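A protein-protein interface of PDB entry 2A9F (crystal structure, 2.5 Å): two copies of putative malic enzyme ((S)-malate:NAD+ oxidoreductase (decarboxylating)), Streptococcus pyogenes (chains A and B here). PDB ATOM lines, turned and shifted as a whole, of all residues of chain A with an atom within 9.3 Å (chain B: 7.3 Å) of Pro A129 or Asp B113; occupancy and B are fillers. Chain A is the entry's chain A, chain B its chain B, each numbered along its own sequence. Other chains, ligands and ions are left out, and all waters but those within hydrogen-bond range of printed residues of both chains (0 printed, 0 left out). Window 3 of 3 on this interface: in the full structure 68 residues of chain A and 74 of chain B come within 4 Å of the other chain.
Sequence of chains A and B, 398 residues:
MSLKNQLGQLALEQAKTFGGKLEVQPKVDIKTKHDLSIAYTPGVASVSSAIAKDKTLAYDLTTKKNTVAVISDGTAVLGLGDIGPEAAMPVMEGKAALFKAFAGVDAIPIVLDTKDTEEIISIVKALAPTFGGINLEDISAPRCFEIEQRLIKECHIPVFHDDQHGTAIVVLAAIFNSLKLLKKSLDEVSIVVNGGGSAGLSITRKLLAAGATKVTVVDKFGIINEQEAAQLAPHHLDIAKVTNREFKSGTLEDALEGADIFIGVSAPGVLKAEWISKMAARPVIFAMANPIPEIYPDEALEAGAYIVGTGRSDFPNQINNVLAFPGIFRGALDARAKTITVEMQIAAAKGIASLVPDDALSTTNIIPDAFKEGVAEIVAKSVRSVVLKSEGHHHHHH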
ATOM      1  N   ILE A  51       6.443  17.463  -1.827  1.00  0.00           N
ATOM      2  CA  ILE A  51       5.043  17.857  -1.961  1.00  0.00           C
ATOM      3  C   ILE A  51       4.201  16.781  -2.644  1.00  0.00           C
ATOM      4  O   ILE A  51       3.027  16.608  -2.332  1.00  0.00           O
ATOM      5  CB  ILE A  51       4.914  19.202  -2.746  1.00  0.00           C
ATOM      6  CG1 ILE A  51       5.735  20.289  -2.055  1.00  0.00           C
ATOM      7  CG2 ILE A  51       3.458  19.667  -2.799  1.00  0.00           C
ATOM      8  CD1 ILE A  51       5.703  21.617  -2.765  1.00  0.00           C
ATOM      9  N   LYS A  55       0.918  16.678   0.097  1.00  0.00           N
ATOM     10  CA  LYS A  55       0.419  17.911  -0.502  1.00  0.00           C
ATOM     11  C   LYS A  55       0.198  19.055   0.476  1.00  0.00           C
ATOM     12  O   LYS A  55      -0.037  20.187   0.058  1.00  0.00           O
ATOM     13  CB  LYS A  55      -0.864  17.616  -1.289  1.00  0.00           C
ATOM     14  CG  LYS A  55      -0.640  16.568  -2.372  1.00  0.00           C
ATOM     15  CD  LYS A  55      -1.873  16.292  -3.219  1.00  0.00           C
ATOM     16  CE  LYS A  55      -1.555  15.225  -4.277  1.00  0.00           C
ATOM     17  NZ  LYS A  55      -2.658  14.984  -5.250  1.00  0.00           N
ATOM     18  N   ALA A  58       2.610  22.000   0.589  1.00  0.00           N
ATOM     19  CA  ALA A  58       2.460  23.128  -0.316  1.00  0.00           C
ATOM     20  C   ALA A  58       2.472  24.438   0.457  1.00  0.00           C
ATOM     21  O   ALA A  58       2.974  25.438  -0.044  1.00  0.00           O
ATOM     22  CB  ALA A  58       1.169  23.012  -1.125  1.00  0.00           C
ATOM     23  N   TYR A  59       1.943  24.428   1.682  1.00  0.00           N
ATOM     24  CA  TYR A  59       1.892  25.637   2.505  1.00  0.00           C
ATOM     25  C   TYR A  59       3.221  26.050   3.107  1.00  0.00           C
ATOM     26  O   TYR A  59       3.384  27.188   3.516  1.00  0.00           O
ATOM     27  CB  TYR A  59       0.868  25.491   3.634  1.00  0.00           C
ATOM     28  CG  TYR A  59      -0.537  25.924   3.256  1.00  0.00           C
ATOM     29  CD1 TYR A  59      -1.530  24.985   2.947  1.00  0.00           C
ATOM     30  CD2 TYR A  59      -0.866  27.276   3.181  1.00  0.00           C
ATOM     31  CE1 TYR A  59      -2.812  25.388   2.574  1.00  0.00           C
ATOM     32  CE2 TYR A  59      -2.124  27.683   2.811  1.00  0.00           C
ATOM     33  CZ  TYR A  59      -3.098  26.737   2.508  1.00  0.00           C
ATOM     34  OH  TYR A  59      -4.344  27.170   2.132  1.00  0.00           O
ATOM     35  N   THR A  62       5.892  26.537  -0.857  1.00  0.00           N
ATOM     36  CA  THR A  62       5.535  27.321  -2.044  1.00  0.00           C
ATOM     37  C   THR A  62       4.944  28.653  -1.631  1.00  0.00           C
ATOM     38  O   THR A  62       4.687  28.877  -0.451  1.00  0.00           O
ATOM     39  CB  THR A  62       4.512  26.589  -2.932  1.00  0.00           C
ATOM     40  OG1 THR A  62       3.201  26.737  -2.380  1.00  0.00           O
ATOM     41  CG2 THR A  62       4.853  25.109  -3.029  1.00  0.00           C
ATOM     42  N   THR A  63       4.727  29.538  -2.594  1.00  0.00           N
ATOM     43  CA  THR A  63       4.166  30.834  -2.260  1.00  0.00           C
ATOM     44  C   THR A  63       2.691  30.773  -1.932  1.00  0.00           C
ATOM     45  O   THR A  63       2.099  31.778  -1.594  1.00  0.00           O
ATOM     46  CB  THR A  63       4.402  31.879  -3.364  1.00  0.00           C
ATOM     47  OG1 THR A  63       3.910  31.395  -4.618  1.00  0.00           O
ATOM     48  CG2 THR A  63       5.868  32.198  -3.462  1.00  0.00           C
ATOM     49  N   LYS A  64       2.100  29.595  -2.016  1.00  0.00           N
ATOM     50  CA  LYS A  64       0.692  29.440  -1.673  1.00  0.00           C
ATOM     51  C   LYS A  64       0.498  29.907  -0.219  1.00  0.00           C
ATOM     52  O   LYS A  64      -0.596  30.304   0.194  1.00  0.00           O
ATOM     53  CB  LYS A  64       0.279  27.964  -1.796  1.00  0.00           C
ATOM     54  CG  LYS A  64      -1.184  27.678  -1.482  1.00  0.00           C
ATOM     55  CD  LYS A  64      -1.442  26.180  -1.427  1.00  0.00           C
ATOM     56  CE  LYS A  64      -2.920  25.866  -1.217  1.00  0.00           C
ATOM     57  NZ  LYS A  64      -3.763  26.290  -2.382  1.00  0.00           N
ATOM     58  N   LYS A  65       1.589  29.847   0.537  1.00  0.00           N
ATOM     59  CA  LYS A  65       1.640  30.225   1.944  1.00  0.00           C
ATOM     60  C   LYS A  65       1.211  31.663   2.265  1.00  0.00           C
ATOM     61  O   LYS A  65       0.531  31.916   3.272  1.00  0.00           O
ATOM     62  CB  LYS A  65       3.075  29.995   2.444  1.00  0.00           C
ATOM     63  CG  LYS A  65       3.281  30.191   3.931  1.00  0.00           C
ATOM     64  CD  LYS A  65       4.724  29.904   4.368  1.00  0.00           C
ATOM     65  CE  LYS A  65       4.904  30.215   5.864  1.00  0.00           C
ATOM     66  NZ  LYS A  65       6.341  30.272   6.310  1.00  0.00           N
ATOM     67  N   THR A  67       0.325  34.038  -0.627  1.00  0.00           N
ATOM     68  CA  THR A  67      -0.233  34.718  -1.790  1.00  0.00           C
ATOM     69  C   THR A  67      -1.710  34.489  -2.052  1.00  0.00           C
ATOM     70  O   THR A  67      -2.202  33.372  -2.111  1.00  0.00           O
ATOM     71  CB  THR A  67       0.527  34.387  -3.105  1.00  0.00           C
ATOM     72  OG1 THR A  67       0.057  33.140  -3.621  1.00  0.00           O
ATOM     73  CG2 THR A  67       2.034  34.319  -2.865  1.00  0.00           C
ATOM     74  N   SER A 122     -15.587  27.808 -12.213  1.00  0.00           N
ATOM     75  CA  SER A 122     -14.795  26.679 -12.663  1.00  0.00           C
ATOM     76  C   SER A 122     -13.346  27.046 -12.984  1.00  0.00           C
ATOM     77  O   SER A 122     -12.451  26.192 -12.908  1.00  0.00           O
ATOM     78  CB  SER A 122     -15.472  26.049 -13.875  1.00  0.00           C
ATOM     79  OG  SER A 122     -16.749  25.565 -13.489  1.00  0.00           O
ATOM     80  N   ILE A 123     -13.125  28.315 -13.337  1.00  0.00           N
ATOM     81  CA  ILE A 123     -11.779  28.828 -13.652  1.00  0.00           C
ATOM     82  C   ILE A 123     -10.984  28.967 -12.360  1.00  0.00           C
ATOM     83  O   ILE A 123      -9.846  28.502 -12.253  1.00  0.00           O
ATOM     84  CB  ILE A 123     -11.842  30.226 -14.329  1.00  0.00           C
ATOM     85  CG1 ILE A 123     -12.020  30.070 -15.842  1.00  0.00           C
ATOM     86  CG2 ILE A 123     -10.576  31.026 -14.013  1.00  0.00           C
ATOM     87  CD1 ILE A 123     -12.612  31.287 -16.505  1.00  0.00           C
ATOM     88  N   VAL A 124     -11.603  29.623 -11.386  1.00  0.00           N
ATOM     89  CA  VAL A 124     -11.006  29.846 -10.083  1.00  0.00           C
ATOM     90  C   VAL A 124     -10.751  28.530  -9.364  1.00  0.00           C
ATOM     91  O   VAL A 124      -9.692  28.343  -8.770  1.00  0.00           O
ATOM     92  CB  VAL A 124     -11.920  30.722  -9.222  1.00  0.00           C
ATOM     93  CG1 VAL A 124     -11.502  30.656  -7.768  1.00  0.00           C
ATOM     94  CG2 VAL A 124     -11.880  32.148  -9.742  1.00  0.00           C
ATOM     95  N   LYS A 125     -11.711  27.613  -9.421  1.00  0.00           N
ATOM     96  CA  LYS A 125     -11.528  26.332  -8.750  1.00  0.00           C
ATOM     97  C   LYS A 125     -10.250  25.681  -9.299  1.00  0.00           C
ATOM     98  O   LYS A 125      -9.496  25.033  -8.575  1.00  0.00           O
ATOM     99  CB  LYS A 125     -12.752  25.427  -8.983  1.00  0.00           C
ATOM    100  CG  LYS A 125     -13.243  24.714  -7.733  1.00  0.00           C
ATOM    101  CD  LYS A 125     -14.613  24.067  -7.950  1.00  0.00           C
ATOM    102  CE  LYS A 125     -14.545  22.953  -8.989  1.00  0.00           C
ATOM    103  NZ  LYS A 125     -15.886  22.476  -9.418  1.00  0.00           N
ATOM    104  N   ALA A 126      -9.999  25.874 -10.585  1.00  0.00           N
ATOM    105  CA  ALA A 126      -8.815  25.296 -11.191  1.00  0.00           C
ATOM    106  C   ALA A 126      -7.538  26.044 -10.771  1.00  0.00           C
ATOM    107  O   ALA A 126      -6.438  25.482 -10.806  1.00  0.00           O
ATOM    108  CB  ALA A 126      -8.970  25.292 -12.703  1.00  0.00           C
ATOM    109  N   LEU A 127      -7.692  27.308 -10.382  1.00  0.00           N
ATOM    110  CA  LEU A 127      -6.569  28.127  -9.950  1.00  0.00           C
ATOM    111  C   LEU A 127      -6.255  27.856  -8.496  1.00  0.00           C
ATOM    112  O   LEU A 127      -5.098  27.906  -8.079  1.00  0.00           O
ATOM    113  CB  LEU A 127      -6.891  29.615 -10.085  1.00  0.00           C
ATOM    114  CG  LEU A 127      -6.991  30.224 -11.474  1.00  0.00           C
ATOM    115  CD1 LEU A 127      -7.589  31.599 -11.386  1.00  0.00           C
ATOM    116  CD2 LEU A 127      -5.614  30.267 -12.100  1.00  0.00           C
ATOM    117  N   ALA A 128      -7.298  27.555  -7.731  1.00  0.00           N
ATOM    118  CA  ALA A 128      -7.168  27.334  -6.297  1.00  0.00           C
ATOM    119  C   ALA A 128      -5.840  26.728  -5.816  1.00  0.00           C
ATOM    120  O   ALA A 128      -5.253  27.217  -4.865  1.00  0.00           O
ATOM    121  CB  ALA A 128      -8.350  26.512  -5.797  1.00  0.00           C
ATOM    122  N   PRO A 129      -5.351  25.665  -6.477  1.00  0.00           N
ATOM    123  CA  PRO A 129      -4.092  25.029  -6.078  1.00  0.00           C
ATOM    124  C   PRO A 129      -2.953  26.018  -5.883  1.00  0.00           C
ATOM    125  O   PRO A 129      -2.171  25.902  -4.941  1.00  0.00           O
ATOM    126  CB  PRO A 129      -3.810  24.074  -7.231  1.00  0.00           C
ATOM    127  CG  PRO A 129      -5.164  23.694  -7.683  1.00  0.00           C
ATOM    128  CD  PRO A 129      -5.912  24.997  -7.666  1.00  0.00           C
ATOM    129  N   THR A 130      -2.884  26.981  -6.796  1.00  0.00           N
ATOM    130  CA  THR A 130      -1.857  28.008  -6.819  1.00  0.00           C
ATOM    131  C   THR A 130      -1.822  28.918  -5.609  1.00  0.00           C
ATOM    132  O   THR A 130      -0.749  29.238  -5.073  1.00  0.00           O
ATOM    133  CB  THR A 130      -2.045  28.925  -8.056  1.00  0.00           C
ATOM    134  OG1 THR A 130      -1.696  28.212  -9.250  1.00  0.00           O
ATOM    135  CG2 THR A 130      -1.187  30.173  -7.942  1.00  0.00           C
ATOM    136  N   PHE A 131      -3.005  29.337  -5.189  1.00  0.00           N
ATOM    137  CA  PHE A 131      -3.117  30.287  -4.116  1.00  0.00           C
ATOM    138  C   PHE A 131      -3.498  29.797  -2.741  1.00  0.00           C
ATOM    139  O   PHE A 131      -3.925  28.654  -2.562  1.00  0.00           O
ATOM    140  CB  PHE A 131      -4.069  31.370  -4.579  1.00  0.00           C
ATOM    141  CG  PHE A 131      -3.652  31.994  -5.869  1.00  0.00           C
ATOM    142  CD1 PHE A 131      -2.676  32.976  -5.894  1.00  0.00           C
ATOM    143  CD2 PHE A 131      -4.206  31.566  -7.073  1.00  0.00           C
ATOM    144  CE1 PHE A 131      -2.255  33.530  -7.101  1.00  0.00           C
ATOM    145  CE2 PHE A 131      -3.792  32.113  -8.287  1.00  0.00           C
ATOM    146  CZ  PHE A 131      -2.815  33.097  -8.303  1.00  0.00           C
ATOM    147  N   GLY A 132      -3.308  30.683  -1.765  1.00  0.00           N
ATOM    148  CA  GLY A 132      -3.650  30.381  -0.395  1.00  0.00           C
ATOM    149  C   GLY A 132      -4.934  31.101  -0.042  1.00  0.00           C
ATOM    150  O   GLY A 132      -5.496  30.893   1.034  1.00  0.00           O
ATOM    151  N   GLY A 133      -5.400  31.949  -0.960  1.00  0.00           N
ATOM    152  CA  GLY A 133      -6.624  32.694  -0.733  1.00  0.00           C
ATOM    153  C   GLY A 133      -7.160  33.406  -1.965  1.00  0.00           C
ATOM    154  O   GLY A 133      -6.394  33.895  -2.796  1.00  0.00           O
ATOM    155  N   ILE A 134      -8.488  33.474  -2.080  1.00  0.00           N
ATOM    156  CA  ILE A 134      -9.126  34.131  -3.212  1.00  0.00           C
ATOM    157  C   ILE A 134      -9.970  35.318  -2.785  1.00  0.00           C
ATOM    158  O   ILE A 134     -10.839  35.177  -1.933  1.00  0.00           O
ATOM    159  CB  ILE A 134     -10.061  33.179  -3.970  1.00  0.00           C
ATOM    160  CG1 ILE A 134      -9.299  31.929  -4.436  1.00  0.00           C
ATOM    161  CG2 ILE A 134     -10.661  33.911  -5.152  1.00  0.00           C
ATOM    162  CD1 ILE A 134      -8.072  32.213  -5.305  1.00  0.00           C
ATOM    163  N   GLU A 154     -17.271  24.758  -2.714  1.00  0.00           N
ATOM    164  CA  GLU A 154     -16.399  23.876  -3.479  1.00  0.00           C
ATOM    165  C   GLU A 154     -14.880  24.047  -3.333  1.00  0.00           C
ATOM    166  O   GLU A 154     -14.130  23.166  -3.747  1.00  0.00           O
ATOM    167  CB  GLU A 154     -16.791  23.949  -4.961  1.00  0.00           C
ATOM    168  CG  GLU A 154     -18.100  23.227  -5.270  1.00  0.00           C
ATOM    169  CD  GLU A 154     -18.717  23.621  -6.603  1.00  0.00           C
ATOM    170  OE1 GLU A 154     -17.991  23.664  -7.618  1.00  0.00           O
ATOM    171  OE2 GLU A 154     -19.941  23.875  -6.633  1.00  0.00           O
ATOM    172  N   CYS A 155     -14.414  25.150  -2.747  1.00  0.00           N
ATOM    173  CA  CYS A 155     -12.971  25.369  -2.592  1.00  0.00           C
ATOM    174  C   CYS A 155     -12.352  24.913  -1.278  1.00  0.00           C
ATOM    175  O   CYS A 155     -13.007  24.894  -0.230  1.00  0.00           O
ATOM    176  CB  CYS A 155     -12.624  26.843  -2.791  1.00  0.00           C
ATOM    177  SG  CYS A 155     -12.434  27.334  -4.499  1.00  0.00           S
ATOM    178  N   HIS A 156     -11.067  24.573  -1.350  1.00  0.00           N
ATOM    179  CA  HIS A 156     -10.307  24.113  -0.186  1.00  0.00           C
ATOM    180  C   HIS A 156      -9.537  25.265   0.464  1.00  0.00           C
ATOM    181  O   HIS A 156      -8.820  25.080   1.451  1.00  0.00           O
ATOM    182  CB  HIS A 156      -9.339  22.992  -0.600  1.00  0.00           C
ATOM    183  CG  HIS A 156     -10.002  21.867  -1.334  1.00  0.00           C
ATOM    184  ND1 HIS A 156     -10.417  21.975  -2.645  1.00  0.00           N
ATOM    185  CD2 HIS A 156     -10.367  20.628  -0.926  1.00  0.00           C
ATOM    186  CE1 HIS A 156     -11.008  20.852  -3.014  1.00  0.00           C
ATOM    187  NE2 HIS A 156     -10.991  20.018  -1.989  1.00  0.00           N
ATOM    188  N   ILE A 157      -9.691  26.455  -0.106  1.00  0.00           N
ATOM    189  CA  ILE A 157      -9.039  27.642   0.413  1.00  0.00           C
ATOM    190  C   ILE A 157     -10.107  28.693   0.615  1.00  0.00           C
ATOM    191  O   ILE A 157     -11.151  28.647  -0.017  1.00  0.00           O
ATOM    192  CB  ILE A 157      -7.959  28.173  -0.552  1.00  0.00           C
ATOM    193  CG1 ILE A 157      -8.540  28.329  -1.963  1.00  0.00           C
ATOM    194  CG2 ILE A 157      -6.762  27.236  -0.545  1.00  0.00           C
ATOM    195  CD1 ILE A 157      -7.582  28.979  -2.957  1.00  0.00           C
ATOM    196  N   SER B  72       1.266  25.579 -15.887  1.00  0.00           N
ATOM    197  CA  SER B  72       1.415  24.131 -15.997  1.00  0.00           C
ATOM    198  C   SER B  72       0.279  23.426 -15.275  1.00  0.00           C
ATOM    199  O   SER B  72      -0.398  24.011 -14.432  1.00  0.00           O
ATOM    200  CB  SER B  72       2.749  23.681 -15.403  1.00  0.00           C
ATOM    201  OG  SER B  72       2.928  24.205 -14.102  1.00  0.00           O
ATOM    202  N   ASP B  73       0.071  22.161 -15.615  1.00  0.00           N
ATOM    203  CA  ASP B  73      -0.981  21.372 -14.998  1.00  0.00           C
ATOM    204  C   ASP B  73      -0.331  20.321 -14.123  1.00  0.00           C
ATOM    205  O   ASP B  73      -0.993  19.399 -13.668  1.00  0.00           O
ATOM    206  CB  ASP B  73      -1.839  20.698 -16.075  1.00  0.00           C
ATOM    207  CG  ASP B  73      -1.011  19.840 -17.033  1.00  0.00           C
ATOM    208  OD1 ASP B  73       0.232  19.829 -16.903  1.00  0.00           O
ATOM    209  OD2 ASP B  73      -1.591  19.176 -17.918  1.00  0.00           O
ATOM    210  N   GLY B  84       0.764  16.396 -10.106  1.00  0.00           N
ATOM    211  CA  GLY B  84      -0.231  17.346  -9.632  1.00  0.00           C
ATOM    212  C   GLY B  84       0.259  18.785  -9.579  1.00  0.00           C
ATOM    213  O   GLY B  84       1.467  19.028  -9.518  1.00  0.00           O
ATOM    214  N   PRO B  85      -0.659  19.764  -9.580  1.00  0.00           N
ATOM    215  CA  PRO B  85      -0.326  21.198  -9.533  1.00  0.00           C
ATOM    216  C   PRO B  85       0.482  21.698  -8.323  1.00  0.00           C
ATOM    217  O   PRO B  85       1.462  22.422  -8.495  1.00  0.00           O
ATOM    218  CB  PRO B  85      -1.697  21.880  -9.637  1.00  0.00           C
ATOM    219  CG  PRO B  85      -2.604  20.899  -8.934  1.00  0.00           C
ATOM    220  CD  PRO B  85      -2.118  19.561  -9.493  1.00  0.00           C
ATOM    221  N   GLU B  86       0.092  21.332  -7.105  1.00  0.00           N
ATOM    222  CA  GLU B  86       0.839  21.814  -5.937  1.00  0.00           C
ATOM    223  C   GLU B  86       2.327  21.477  -6.014  1.00  0.00           C
ATOM    224  O   GLU B  86       3.176  22.328  -5.761  1.00  0.00           O
ATOM    225  CB  GLU B  86       0.265  21.262  -4.623  1.00  0.00           C
ATOM    226  CG  GLU B  86      -1.078  21.856  -4.215  1.00  0.00           C
ATOM    227  CD  GLU B  86      -2.274  21.057  -4.732  1.00  0.00           C
ATOM    228  OE1 GLU B  86      -2.112  20.268  -5.706  1.00  0.00           O
ATOM    229  OE2 GLU B  86      -3.382  21.230  -4.165  1.00  0.00           O
ATOM    230  N   MET B  89       4.218  23.573  -8.521  1.00  0.00           N
ATOM    231  CA  MET B  89       4.413  24.966  -8.124  1.00  0.00           C
ATOM    232  C   MET B  89       5.866  25.363  -7.839  1.00  0.00           C
ATOM    233  O   MET B  89       6.300  26.461  -8.204  1.00  0.00           O
ATOM    234  CB  MET B  89       3.516  25.279  -6.918  1.00  0.00           C
ATOM    235  CG  MET B  89       3.289  26.753  -6.668  1.00  0.00           C
ATOM    236  SD  MET B  89       2.396  27.626  -7.967  1.00  0.00           S
ATOM    237  CE  MET B  89       2.232  29.135  -7.216  1.00  0.00           C
ATOM    238  N   ILE B 110       1.530  29.831 -12.054  1.00  0.00           N
ATOM    239  CA  ILE B 110       0.129  29.458 -11.905  1.00  0.00           C
ATOM    240  C   ILE B 110      -0.096  27.986 -12.222  1.00  0.00           C
ATOM    241  O   ILE B 110       0.149  27.539 -13.339  1.00  0.00           O
ATOM    242  CB  ILE B 110      -0.755  30.287 -12.834  1.00  0.00           C
ATOM    243  CG1 ILE B 110      -0.935  31.692 -12.264  1.00  0.00           C
ATOM    244  CG2 ILE B 110      -2.083  29.600 -13.037  1.00  0.00           C
ATOM    245  CD1 ILE B 110      -1.865  32.533 -13.077  1.00  0.00           C
ATOM    246  N   VAL B 111      -0.559  27.223 -11.246  1.00  0.00           N
ATOM    247  CA  VAL B 111      -0.818  25.814 -11.502  1.00  0.00           C
ATOM    248  C   VAL B 111      -2.323  25.567 -11.632  1.00  0.00           C
ATOM    249  O   VAL B 111      -3.128  26.339 -11.101  1.00  0.00           O
ATOM    250  CB  VAL B 111      -0.224  24.959 -10.397  1.00  0.00           C
ATOM    251  CG1 VAL B 111       1.296  25.026 -10.471  1.00  0.00           C
ATOM    252  CG2 VAL B 111      -0.725  25.455  -9.055  1.00  0.00           C
ATOM    253  N   LEU B 112      -2.701  24.505 -12.347  1.00  0.00           N
ATOM    254  CA  LEU B 112      -4.122  24.186 -12.571  1.00  0.00           C
ATOM    255  C   LEU B 112      -4.595  22.795 -12.133  1.00  0.00           C
ATOM    256  O   LEU B 112      -3.935  21.780 -12.371  1.00  0.00           O
ATOM    257  CB  LEU B 112      -4.462  24.363 -14.054  1.00  0.00           C
ATOM    258  CG  LEU B 112      -4.333  25.757 -14.667  1.00  0.00           C
ATOM    259  CD1 LEU B 112      -4.513  25.680 -16.176  1.00  0.00           C
ATOM    260  CD2 LEU B 112      -5.369  26.670 -14.043  1.00  0.00           C
ATOM    261  N   ASP B 113      -5.771  22.752 -11.520  1.00  0.00           N
ATOM    262  CA  ASP B 113      -6.353  21.495 -11.066  1.00  0.00           C
ATOM    263  C   ASP B 113      -7.283  20.870 -12.118  1.00  0.00           C
ATOM    264  O   ASP B 113      -8.464  20.682 -11.859  1.00  0.00           O
ATOM    265  CB  ASP B 113      -7.141  21.727  -9.765  1.00  0.00           C
ATOM    266  CG  ASP B 113      -7.663  20.430  -9.139  1.00  0.00           C
ATOM    267  OD1 ASP B 113      -8.651  20.511  -8.378  1.00  0.00           O
ATOM    268  OD2 ASP B 113      -7.091  19.341  -9.390  1.00  0.00           O
ATOM    269  N   THR B 114      -6.764  20.588 -13.312  1.00  0.00           N
ATOM    270  CA  THR B 114      -7.541  19.928 -14.373  1.00  0.00           C
ATOM    271  C   THR B 114      -6.565  19.439 -15.418  1.00  0.00           C
ATOM    272  O   THR B 114      -5.427  19.898 -15.469  1.00  0.00           O
ATOM    273  CB  THR B 114      -8.548  20.838 -15.121  1.00  0.00           C
ATOM    274  OG1 THR B 114      -7.837  21.823 -15.875  1.00  0.00           O
ATOM    275  CG2 THR B 114      -9.515  21.507 -14.161  1.00  0.00           C
ATOM    276  N   LYS B 115      -7.017  18.517 -16.259  1.00  0.00           N
ATOM    277  CA  LYS B 115      -6.172  17.975 -17.304  1.00  0.00           C
ATOM    278  C   LYS B 115      -6.902  17.948 -18.637  1.00  0.00           C
ATOM    279  O   LYS B 115      -6.297  17.709 -19.681  1.00  0.00           O
ATOM    280  CB  LYS B 115      -5.715  16.566 -16.923  1.00  0.00           C
ATOM    281  CG  LYS B 115      -5.064  16.487 -15.551  1.00  0.00           C
ATOM    282  CD  LYS B 115      -4.452  15.125 -15.292  1.00  0.00           C
ATOM    283  CE  LYS B 115      -3.957  15.022 -13.858  1.00  0.00           C
ATOM    284  NZ  LYS B 115      -3.310  13.713 -13.547  1.00  0.00           N
ATOM    285  N   ASP B 116      -8.209  18.193 -18.590  1.00  0.00           N
ATOM    286  CA  ASP B 116      -9.049  18.200 -19.786  1.00  0.00           C
ATOM    287  C   ASP B 116      -8.556  19.303 -20.716  1.00  0.00           C
ATOM    288  O   ASP B 116      -8.662  20.489 -20.389  1.00  0.00           O
ATOM    289  CB  ASP B 116     -10.504  18.457 -19.387  1.00  0.00           C
ATOM    290  CG  ASP B 116     -11.477  18.214 -20.524  1.00  0.00           C
ATOM    291  OD1 ASP B 116     -11.683  17.036 -20.909  1.00  0.00           O
ATOM    292  OD2 ASP B 116     -12.035  19.209 -21.032  1.00  0.00           O
ATOM    293  N   GLU B 119     -10.507  22.436 -21.220  1.00  0.00           N
ATOM    294  CA  GLU B 119     -10.574  23.204 -19.982  1.00  0.00           C
ATOM    295  C   GLU B 119      -9.345  24.105 -19.865  1.00  0.00           C
ATOM    296  O   GLU B 119      -9.455  25.277 -19.552  1.00  0.00           O
ATOM    297  CB  GLU B 119     -10.632  22.249 -18.790  1.00  0.00           C
ATOM    298  CG  GLU B 119     -12.030  21.891 -18.352  1.00  0.00           C
ATOM    299  CD  GLU B 119     -12.539  22.854 -17.302  1.00  0.00           C
ATOM    300  OE1 GLU B 119     -13.723  23.262 -17.379  1.00  0.00           O
ATOM    301  OE2 GLU B 119     -11.742  23.198 -16.393  1.00  0.00           O
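Hydrophobic or aromatic side chains of chain A that line the printed part of chain B: Ile A51, Ala A58, Leu A127 and Pro A129. Among the printed residues, 15 pairs touch across the chains. Among the printed residues, no Asp or Glu carboxylate lies within 4 Å of a Lys or Arg side-chain nitrogen of the other chain.
The backbone NH (N) of Asp B113 sits at hydrogen-bond distance from the backbone carbonyl oxygen (O) of Ala A126, at 2.9 Å. OG1 of Thr A130 is in hydrogen-bond range of N of Val B111, at 2.5 Å. The backbone carbonyl oxygen (O) of Val B111 sits close to the backbone carbonyl oxygen (O) of Ala A126, at 3.4 Å.
No position is printed for both chains.
Among the printed residues, pairs that only touch across the chains: Ile A51 with Glu B86, Ala A58 with Glu B86, Thr A62 with Met B89, Thr A63 with Met B89, Ala A126 with Leu B112, Leu A127 with Ile B110, Leu A127 with Val B111, Pro A129 with Pro B85, Pro A129 with Val B111, Pro A129 with Asp B113, Thr A130 with Met B89 and Thr A130 with Ile B110.
OG1 of Thr A62 is in hydrogen-bond range of O of Ala A58, 2.7 Å away. The backbone NH (N) of Lys A64 sits close to the side-chain hydroxyl (OG1) of Thr A62, at 3.1 Å. The backbone carbonyl oxygen (O) of Thr A63 lies close to the side-chain hydroxyl (OG1) of Thr A67 (3.2 Å). The backbone carbonyl oxygen (O) of Pro A129 lies within hydrogen-bond range of the side-chain amino group (NZ) of Lys A64 (3.0 Å). The backbone carbonyl oxygen (O) of Ile B110 sits at hydrogen-bond distance from the backbone NH (N) of Ser B72, at 3.4 Å. The backbone carbonyl oxygen (O) of Ser B72 is in hydrogen-bond range of the backbone NH (N) of Leu B112 (3.1 Å).
Of the printed residues of chain B, Thr A63 touches Met B89 (3.8 Å). No residue of chain B comes within 4 Å of Ala A128. Of chain B, only Pro B85, Val B111 and Asp B113 come within 4 Å of Pro A129. Asp B73 touches none of the printed residues of chain A. Of the printed residues of chain A, Glu B86 touches Ile A51 (3.9 Å) and Ala A58 (3.99 Å). Asp B113 touches just these residues of chain A: Ala A126 and Pro A129. The nearest residue of chain B that does not touch Pro A129 is Glu B86 (4.2 Å). The nearest residue of chain A that does not touch Asp B113 is Lys A125 (4.2 Å).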
